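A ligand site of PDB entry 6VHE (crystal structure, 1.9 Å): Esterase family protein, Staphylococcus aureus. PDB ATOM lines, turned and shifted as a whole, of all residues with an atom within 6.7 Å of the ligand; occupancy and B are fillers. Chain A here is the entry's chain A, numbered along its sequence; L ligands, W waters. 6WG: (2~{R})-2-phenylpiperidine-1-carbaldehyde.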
ATOM      1  N   HIS A  48      19.953 -20.875  17.800  1.00  0.00           N
ATOM      2  CA  HIS A  48      19.670 -21.587  19.045  1.00  0.00           C
ATOM      3  C   HIS A  48      20.466 -22.898  19.156  1.00  0.00           C
ATOM      4  O   HIS A  48      20.934 -23.457  18.167  1.00  0.00           O
ATOM      5  CB  HIS A  48      18.181 -21.886  19.148  1.00  0.00           C
ATOM      6  CG  HIS A  48      17.679 -22.811  18.089  1.00  0.00           C
ATOM      7  ND1 HIS A  48      17.908 -24.180  18.128  1.00  0.00           N
ATOM      8  CD2 HIS A  48      16.973 -22.589  16.961  1.00  0.00           C
ATOM      9  CE1 HIS A  48      17.375 -24.740  17.059  1.00  0.00           C
ATOM     10  NE2 HIS A  48      16.786 -23.799  16.343  1.00  0.00           N
ATOM     11  N   GLY A  49      20.586 -23.385  20.400  1.00  0.00           N
ATOM     12  CA  GLY A  49      21.199 -24.663  20.686  1.00  0.00           C
ATOM     13  C   GLY A  49      20.205 -25.811  20.569  1.00  0.00           C
ATOM     14  O   GLY A  49      19.022 -25.629  20.251  1.00  0.00           O
ATOM     15  N   LEU A  50      20.696 -27.021  20.822  1.00  0.00           N
ATOM     16  CA  LEU A  50      19.878 -28.209  20.634  1.00  0.00           C
ATOM     17  C   LEU A  50      18.776 -28.244  21.673  1.00  0.00           C
ATOM     18  O   LEU A  50      19.027 -28.043  22.858  1.00  0.00           O
ATOM     19  CB  LEU A  50      20.726 -29.474  20.721  1.00  0.00           C
ATOM     20  CG  LEU A  50      19.983 -30.808  20.523  1.00  0.00           C
ATOM     21  CD1 LEU A  50      19.466 -30.936  19.096  1.00  0.00           C
ATOM     22  CD2 LEU A  50      20.889 -32.001  20.878  1.00  0.00           C
ATOM     23  N   SER A  51      17.542 -28.471  21.215  1.00  0.00           N
ATOM     24  CA  SER A  51      16.283 -28.542  21.975  1.00  0.00           C
ATOM     25  C   SER A  51      15.637 -27.163  22.113  1.00  0.00           C
ATOM     26  O   SER A  51      14.485 -27.084  22.539  1.00  0.00           O
ATOM     27  CB  SER A  51      16.436 -29.182  23.366  1.00  0.00           C
ATOM     28  OG  SER A  51      16.948 -28.244  24.301  1.00  0.00           O
ATOM     29  N   HIS A 122      24.645 -20.340  20.486  1.00  0.00           N
ATOM     30  CA  HIS A 122      25.196 -21.125  21.593  1.00  0.00           C
ATOM     31  C   HIS A 122      25.052 -22.624  21.349  1.00  0.00           C
ATOM     32  O   HIS A 122      24.103 -23.082  20.686  1.00  0.00           O
ATOM     33  CB  HIS A 122      24.535 -20.733  22.937  1.00  0.00           C
ATOM     34  CG  HIS A 122      23.097 -21.128  23.048  1.00  0.00           C
ATOM     35  ND1 HIS A 122      22.076 -20.310  22.629  1.00  0.00           N
ATOM     36  CD2 HIS A 122      22.510 -22.268  23.502  1.00  0.00           C
ATOM     37  CE1 HIS A 122      20.909 -20.920  22.830  1.00  0.00           C
ATOM     38  NE2 HIS A 122      21.155 -22.103  23.350  1.00  0.00           N
ATOM     39  N   SER A 123      26.022 -23.395  21.860  1.00  0.00           N
ATOM     40  CA  SER A 123      26.100 -24.855  21.748  1.00  0.00           C
ATOM     41  C   SER A 123      26.023 -25.305  20.293  1.00  0.00           C
ATOM     42  O   SER A 123      26.908 -24.984  19.494  1.00  0.00           O
ATOM     43  CB  SER A 123      25.003 -25.534  22.592  1.00  0.00           C
ATOM     44  OG  SER A 123      25.231 -26.931  22.738  1.00  0.00           O
ATOM     45  N   MET A 124      24.968 -26.054  19.931  1.00  0.00           N
ATOM     46  CA  MET A 124      24.729 -26.377  18.517  1.00  0.00           C
ATOM     47  C   MET A 124      24.702 -25.126  17.658  1.00  0.00           C
ATOM     48  O   MET A 124      25.107 -25.156  16.485  1.00  0.00           O
ATOM     49  CB  MET A 124      23.419 -27.154  18.368  1.00  0.00           C
ATOM     50  CG  MET A 124      23.090 -27.625  16.946  1.00  0.00           C
ATOM     51  SD  MET A 124      21.479 -28.478  16.849  1.00  0.00           S
ATOM     52  CE  MET A 124      20.385 -27.042  16.795  1.00  0.00           C
ATOM     53  N   GLY A 125      24.230 -24.000  18.211  1.00  0.00           N
ATOM     54  CA  GLY A 125      24.231 -22.761  17.457  1.00  0.00           C
ATOM     55  C   GLY A 125      25.580 -22.081  17.409  1.00  0.00           C
ATOM     56  O   GLY A 125      25.816 -21.269  16.501  1.00  0.00           O
ATOM     57  N   SER A 147      29.717 -21.033  24.036  1.00  0.00           N
ATOM     58  CA  SER A 147      29.674 -22.399  24.567  1.00  0.00           C
ATOM     59  C   SER A 147      29.543 -23.404  23.431  1.00  0.00           C
ATOM     60  O   SER A 147      28.732 -24.331  23.473  1.00  0.00           O
ATOM     61  CB  SER A 147      28.533 -22.557  25.568  1.00  0.00           C
ATOM     62  OG  SER A 147      28.488 -21.460  26.463  1.00  0.00           O
ATOM     63  N   VAL A 149      30.336 -26.143  20.250  1.00  0.00           N
ATOM     64  CA  VAL A 149      30.968 -27.418  19.969  1.00  0.00           C
ATOM     65  C   VAL A 149      31.862 -27.223  18.756  1.00  0.00           C
ATOM     66  O   VAL A 149      31.378 -26.894  17.669  1.00  0.00           O
ATOM     67  CB  VAL A 149      29.932 -28.519  19.697  1.00  0.00           C
ATOM     68  CG1 VAL A 149      30.651 -29.846  19.422  1.00  0.00           C
ATOM     69  CG2 VAL A 149      28.968 -28.616  20.837  1.00  0.00           C
ATOM     70  N   GLU A 151      34.730 -29.603  18.219  1.00  0.00           N
ATOM     71  CA  GLU A 151      34.968 -30.986  17.824  1.00  0.00           C
ATOM     72  C   GLU A 151      33.614 -31.624  17.554  1.00  0.00           C
ATOM     73  O   GLU A 151      32.960 -32.112  18.483  1.00  0.00           O
ATOM     74  CB  GLU A 151      35.736 -31.744  18.898  1.00  0.00           C
ATOM     75  CG  GLU A 151      36.114 -33.141  18.440  1.00  0.00           C
ATOM     76  CD  GLU A 151      36.490 -33.156  16.960  1.00  0.00           C
ATOM     77  OE1 GLU A 151      35.642 -33.556  16.120  1.00  0.00           O
ATOM     78  OE2 GLU A 151      37.635 -32.755  16.655  1.00  0.00           O
ATOM     79  N   ALA A 152      33.203 -31.638  16.284  1.00  0.00           N
ATOM     80  CA  ALA A 152      31.854 -32.072  15.944  1.00  0.00           C
ATOM     81  C   ALA A 152      31.591 -33.535  16.245  1.00  0.00           C
ATOM     82  O   ALA A 152      30.426 -33.925  16.360  1.00  0.00           O
ATOM     83  CB  ALA A 152      31.559 -31.811  14.464  1.00  0.00           C
ATOM     84  N   GLN A 153      32.630 -34.373  16.357  1.00  0.00           N
ATOM     85  CA  GLN A 153      32.364 -35.779  16.658  1.00  0.00           C
ATOM     86  C   GLN A 153      31.646 -35.954  17.994  1.00  0.00           C
ATOM     87  O   GLN A 153      31.087 -37.028  18.238  1.00  0.00           O
ATOM     88  CB  GLN A 153      33.668 -36.584  16.656  1.00  0.00           C
ATOM     89  CG  GLN A 153      33.471 -38.093  16.523  1.00  0.00           C
ATOM     90  CD  GLN A 153      32.700 -38.496  15.278  1.00  0.00           C
ATOM     91  OE1 GLN A 153      33.099 -38.171  14.156  1.00  0.00           O
ATOM     92  NE2 GLN A 153      31.587 -39.203  15.466  1.00  0.00           N
ATOM     93  N   ASN A 154      31.632 -34.922  18.823  1.00  0.00           N
ATOM     94  CA  ASN A 154      30.986 -34.970  20.137  1.00  0.00           C
ATOM     95  C   ASN A 154      29.491 -34.668  20.064  1.00  0.00           C
ATOM     96  O   ASN A 154      28.696 -35.357  20.703  1.00  0.00           O
ATOM     97  CB  ASN A 154      31.705 -33.999  21.073  1.00  0.00           C
ATOM     98  CG  ASN A 154      33.058 -34.521  21.526  1.00  0.00           C
ATOM     99  OD1 ASN A 154      33.441 -35.657  21.201  1.00  0.00           O
ATOM    100  ND2 ASN A 154      33.804 -33.696  22.257  1.00  0.00           N
ATOM    101  N   LEU A 155      29.094 -33.656  19.288  1.00  0.00           N
ATOM    102  CA  LEU A 155      27.674 -33.440  19.035  1.00  0.00           C
ATOM    103  C   LEU A 155      27.059 -34.648  18.344  1.00  0.00           C
ATOM    104  O   LEU A 155      25.993 -35.126  18.742  1.00  0.00           O
ATOM    105  CB  LEU A 155      27.450 -32.159  18.211  1.00  0.00           C
ATOM    106  CG  LEU A 155      26.019 -31.666  17.926  1.00  0.00           C
ATOM    107  CD1 LEU A 155      25.181 -31.393  19.193  1.00  0.00           C
ATOM    108  CD2 LEU A 155      26.046 -30.430  17.053  1.00  0.00           C
ATOM    109  N   MET A 156      27.723 -35.152  17.312  1.00  0.00           N
ATOM    110  CA  MET A 156      27.186 -36.273  16.551  1.00  0.00           C
ATOM    111  C   MET A 156      26.976 -37.497  17.430  1.00  0.00           C
ATOM    112  O   MET A 156      25.968 -38.195  17.316  1.00  0.00           O
ATOM    113  CB  MET A 156      28.091 -36.589  15.366  1.00  0.00           C
ATOM    114  CG  MET A 156      28.150 -35.474  14.320  1.00  0.00           C
ATOM    115  SD  MET A 156      26.580 -34.589  14.222  1.00  0.00           S
ATOM    116  CE  MET A 156      27.046 -33.092  13.365  1.00  0.00           C
ATOM    117  N   LEU A 158      26.647 -37.507  20.727  1.00  0.00           N
ATOM    118  CA  LEU A 158      25.787 -37.224  21.870  1.00  0.00           C
ATOM    119  C   LEU A 158      24.516 -38.067  21.826  1.00  0.00           C
ATOM    120  O   LEU A 158      23.900 -38.226  20.768  1.00  0.00           O
ATOM    121  CB  LEU A 158      25.446 -35.717  21.879  1.00  0.00           C
ATOM    122  CG  LEU A 158      24.478 -35.108  22.884  1.00  0.00           C
ATOM    123  CD1 LEU A 158      25.149 -34.888  24.236  1.00  0.00           C
ATOM    124  CD2 LEU A 158      23.963 -33.805  22.344  1.00  0.00           C
ATOM    125  N   TRP A 160      21.562 -37.398  23.102  1.00  0.00           N
ATOM    126  CA  TRP A 160      20.547 -36.470  23.585  1.00  0.00           C
ATOM    127  C   TRP A 160      19.137 -36.971  23.248  1.00  0.00           C
ATOM    128  O   TRP A 160      18.923 -37.749  22.314  1.00  0.00           O
ATOM    129  CB  TRP A 160      20.768 -35.090  22.971  1.00  0.00           C
ATOM    130  CG  TRP A 160      19.748 -34.024  23.356  1.00  0.00           C
ATOM    131  CD1 TRP A 160      18.567 -33.735  22.714  1.00  0.00           C
ATOM    132  CD2 TRP A 160      19.855 -33.095  24.441  1.00  0.00           C
ATOM    133  NE1 TRP A 160      17.928 -32.696  23.343  1.00  0.00           N
ATOM    134  CE2 TRP A 160      18.692 -32.289  24.407  1.00  0.00           C
ATOM    135  CE3 TRP A 160      20.798 -32.873  25.452  1.00  0.00           C
ATOM    136  CZ2 TRP A 160      18.463 -31.272  25.337  1.00  0.00           C
ATOM    137  CZ3 TRP A 160      20.569 -31.853  26.373  1.00  0.00           C
ATOM    138  CH2 TRP A 160      19.410 -31.069  26.309  1.00  0.00           C
ATOM    139  N   ASP A 207      31.576 -25.041  32.094  1.00  0.00           N
ATOM    140  CA  ASP A 207      30.938 -25.718  30.975  1.00  0.00           C
ATOM    141  C   ASP A 207      31.749 -26.951  30.600  1.00  0.00           C
ATOM    142  O   ASP A 207      32.974 -26.884  30.481  1.00  0.00           O
ATOM    143  CB  ASP A 207      30.848 -24.776  29.779  1.00  0.00           C
ATOM    144  CG  ASP A 207      29.866 -25.251  28.732  1.00  0.00           C
ATOM    145  OD1 ASP A 207      29.915 -26.440  28.317  1.00  0.00           O
ATOM    146  OD2 ASP A 207      29.042 -24.429  28.313  1.00  0.00           O
ATOM    147  N   PHE A 208      31.063 -28.079  30.399  1.00  0.00           N
ATOM    148  CA  PHE A 208      31.796 -29.274  30.003  1.00  0.00           C
ATOM    149  C   PHE A 208      32.407 -29.134  28.616  1.00  0.00           C
ATOM    150  O   PHE A 208      33.262 -29.948  28.245  1.00  0.00           O
ATOM    151  CB  PHE A 208      30.891 -30.498  30.087  1.00  0.00           C
ATOM    152  CG  PHE A 208      29.664 -30.413  29.234  1.00  0.00           C
ATOM    153  CD1 PHE A 208      28.576 -29.630  29.625  1.00  0.00           C
ATOM    154  CD2 PHE A 208      29.592 -31.108  28.039  1.00  0.00           C
ATOM    155  CE1 PHE A 208      27.445 -29.546  28.841  1.00  0.00           C
ATOM    156  CE2 PHE A 208      28.465 -31.036  27.261  1.00  0.00           C
ATOM    157  CZ  PHE A 208      27.390 -30.258  27.650  1.00  0.00           C
ATOM    158  N   LEU A 209      32.024 -28.127  27.839  1.00  0.00           N
ATOM    159  CA  LEU A 209      32.654 -27.852  26.559  1.00  0.00           C
ATOM    160  C   LEU A 209      33.881 -26.942  26.681  1.00  0.00           C
ATOM    161  O   LEU A 209      34.440 -26.549  25.657  1.00  0.00           O
ATOM    162  CB  LEU A 209      31.644 -27.233  25.602  1.00  0.00           C
ATOM    163  CG  LEU A 209      30.597 -28.223  25.104  1.00  0.00           C
ATOM    164  CD1 LEU A 209      29.482 -27.518  24.314  1.00  0.00           C
ATOM    165  CD2 LEU A 209      31.287 -29.299  24.258  1.00  0.00           C
ATOM    166  N   ASP A 212      37.052 -28.336  25.047  1.00  0.00           N
ATOM    167  CA  ASP A 212      36.792 -28.287  23.615  1.00  0.00           C
ATOM    168  C   ASP A 212      37.043 -26.880  23.067  1.00  0.00           C
ATOM    169  O   ASP A 212      37.663 -26.713  22.002  1.00  0.00           O
ATOM    170  CB  ASP A 212      35.341 -28.736  23.372  1.00  0.00           C
ATOM    171  CG  ASP A 212      34.929 -28.706  21.915  1.00  0.00           C
ATOM    172  OD1 ASP A 212      34.556 -29.785  21.393  1.00  0.00           O
ATOM    173  OD2 ASP A 212      34.910 -27.623  21.303  1.00  0.00           O
ATOM    174  N   HIS A 236      26.740 -24.313  31.328  1.00  0.00           N
ATOM    175  CA  HIS A 236      26.095 -24.492  30.026  1.00  0.00           C
ATOM    176  C   HIS A 236      24.591 -24.248  30.166  1.00  0.00           C
ATOM    177  O   HIS A 236      23.781 -25.174  30.144  1.00  0.00           O
ATOM    178  CB  HIS A 236      26.413 -25.893  29.498  1.00  0.00           C
ATOM    179  CG  HIS A 236      26.128 -26.057  28.036  1.00  0.00           C
ATOM    180  ND1 HIS A 236      27.053 -25.791  27.057  1.00  0.00           N
ATOM    181  CD2 HIS A 236      24.993 -26.428  27.398  1.00  0.00           C
ATOM    182  CE1 HIS A 236      26.519 -26.004  25.875  1.00  0.00           C
ATOM    183  NE2 HIS A 236      25.255 -26.370  26.048  1.00  0.00           N
ATOM    184  N   TRP A 241      24.180 -17.643  28.991  1.00  0.00           N
ATOM    185  CA  TRP A 241      24.018 -17.065  27.661  1.00  0.00           C
ATOM    186  C   TRP A 241      23.344 -15.681  27.714  1.00  0.00           C
ATOM    187  O   TRP A 241      23.638 -14.827  26.867  1.00  0.00           O
ATOM    188  CB  TRP A 241      23.249 -18.036  26.754  1.00  0.00           C
ATOM    189  CG  TRP A 241      24.034 -19.319  26.606  1.00  0.00           C
ATOM    190  CD1 TRP A 241      25.379 -19.444  26.408  1.00  0.00           C
ATOM    191  CD2 TRP A 241      23.522 -20.664  26.694  1.00  0.00           C
ATOM    192  NE1 TRP A 241      25.737 -20.783  26.346  1.00  0.00           N
ATOM    193  CE2 TRP A 241      24.614 -21.539  26.526  1.00  0.00           C
ATOM    194  CE3 TRP A 241      22.242 -21.205  26.874  1.00  0.00           C
ATOM    195  CZ2 TRP A 241      24.466 -22.927  26.550  1.00  0.00           C
ATOM    196  CZ3 TRP A 241      22.107 -22.581  26.914  1.00  0.00           C
ATOM    197  CH2 TRP A 241      23.209 -23.427  26.747  1.00  0.00           C
HETATM  198  C4  6WG L   1      26.687 -30.878  23.276  1.00  0.00           C
HETATM  199  C7  6WG L   1      25.373 -30.224  23.681  1.00  0.00           C
HETATM  200  C6  6WG L   1      28.668 -32.040  24.026  1.00  0.00           C
HETATM  201  C9  6WG L   1      24.114 -29.555  25.576  1.00  0.00           C
HETATM  202  C8  6WG L   1      25.462 -29.316  24.896  1.00  0.00           C
HETATM  203  C1  6WG L   1      29.086 -32.192  22.721  1.00  0.00           C
HETATM  204  C2  6WG L   1      28.293 -31.691  21.707  1.00  0.00           C
HETATM  205  C3  6WG L   1      27.091 -31.049  21.973  1.00  0.00           C
HETATM  206  C5  6WG L   1      27.466 -31.398  24.293  1.00  0.00           C
HETATM  207  C10 6WG L   1      23.026 -30.120  24.629  1.00  0.00           C
HETATM  208  C11 6WG L   1      23.136 -29.856  23.115  1.00  0.00           C
HETATM  209  N1  6WG L   1      24.491 -29.541  22.722  1.00  0.00           N
HETATM  210  C12 6WG L   1      24.655 -28.133  22.374  1.00  0.00           C
HETATM  211  O1  6WG L   1      23.597 -27.503  21.773  1.00  0.00           O
HETATM  212  O   HOH W   1      22.892 -26.932  24.955  1.00  0.00           O
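The side-chain hydroxyl (OG) of Ser 123 is bonded to a carbon (C12) of the ligand, 1.4 Å away.
The backbone NH (N) of Met 124 sits at hydrogen-bond distance from an oxygen (O1) of the ligand (2.7 Å).
The backbone NH (N) of Leu 50 is in hydrogen-bond range of an oxygen (O1) of the ligand.
A ring nitrogen (NE2) of His 236 is in hydrogen-bond range of the side-chain hydroxyl (OG) of Ser 123, at 3.4 Å.
O of Ser 147 sits close to N of Ser 123 (3.3 Å).
A ring nitrogen (ND1) of His 236 is in hydrogen-bond range of the side-chain carboxylate of Asp 207 (2.7 Å).
The side-chain carboxylate (OD1) of Asp 207 sits at hydrogen-bond distance from the backbone NH (N) of Leu 209 (2.7 Å).
The backbone NH of Gly 49 is in hydrogen-bond range of a ring nitrogen (NE2) of His 122 (3.3 Å).
Gly 49 touches the ligand (CA to O1, 3.9 Å).
CG2 of Val 149 touches C2 of the ligand, 3.3 Å away.
CB of Asn 154 touches C1 of the ligand (3.6 Å).
Leu 155 touches the ligand.
Trp 160 touches the ligand (CZ3 to C10, 3.5 Å).
Phe 208 touches the ligand.
CD2 of Leu 209 touches C6 of the ligand, 3.8 Å away.
NE2 of His 236 touches C8 of the ligand, 3.2 Å away.
Hydrophobic or aromatic side chains within 4 Å of the ligand: Leu 50, Met 124, Val 149, Leu 155, Trp 160, Phe 208, Leu 209 and His 236.
Of the 24 residues printed, 11 come within 4 Å of the ligand.
Along chain A the residues within 4 Å of the ligand span positions 49 to 236.
The nearest printed residue that does not touch the ligand is Leu 158 (4.1 Å).
Water W1 lies within hydrogen-bond range of NE2 of His 236 (2.7 Å), OG of Ser 123 (3.2 Å) and O1 of the ligand (3.3 Å).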
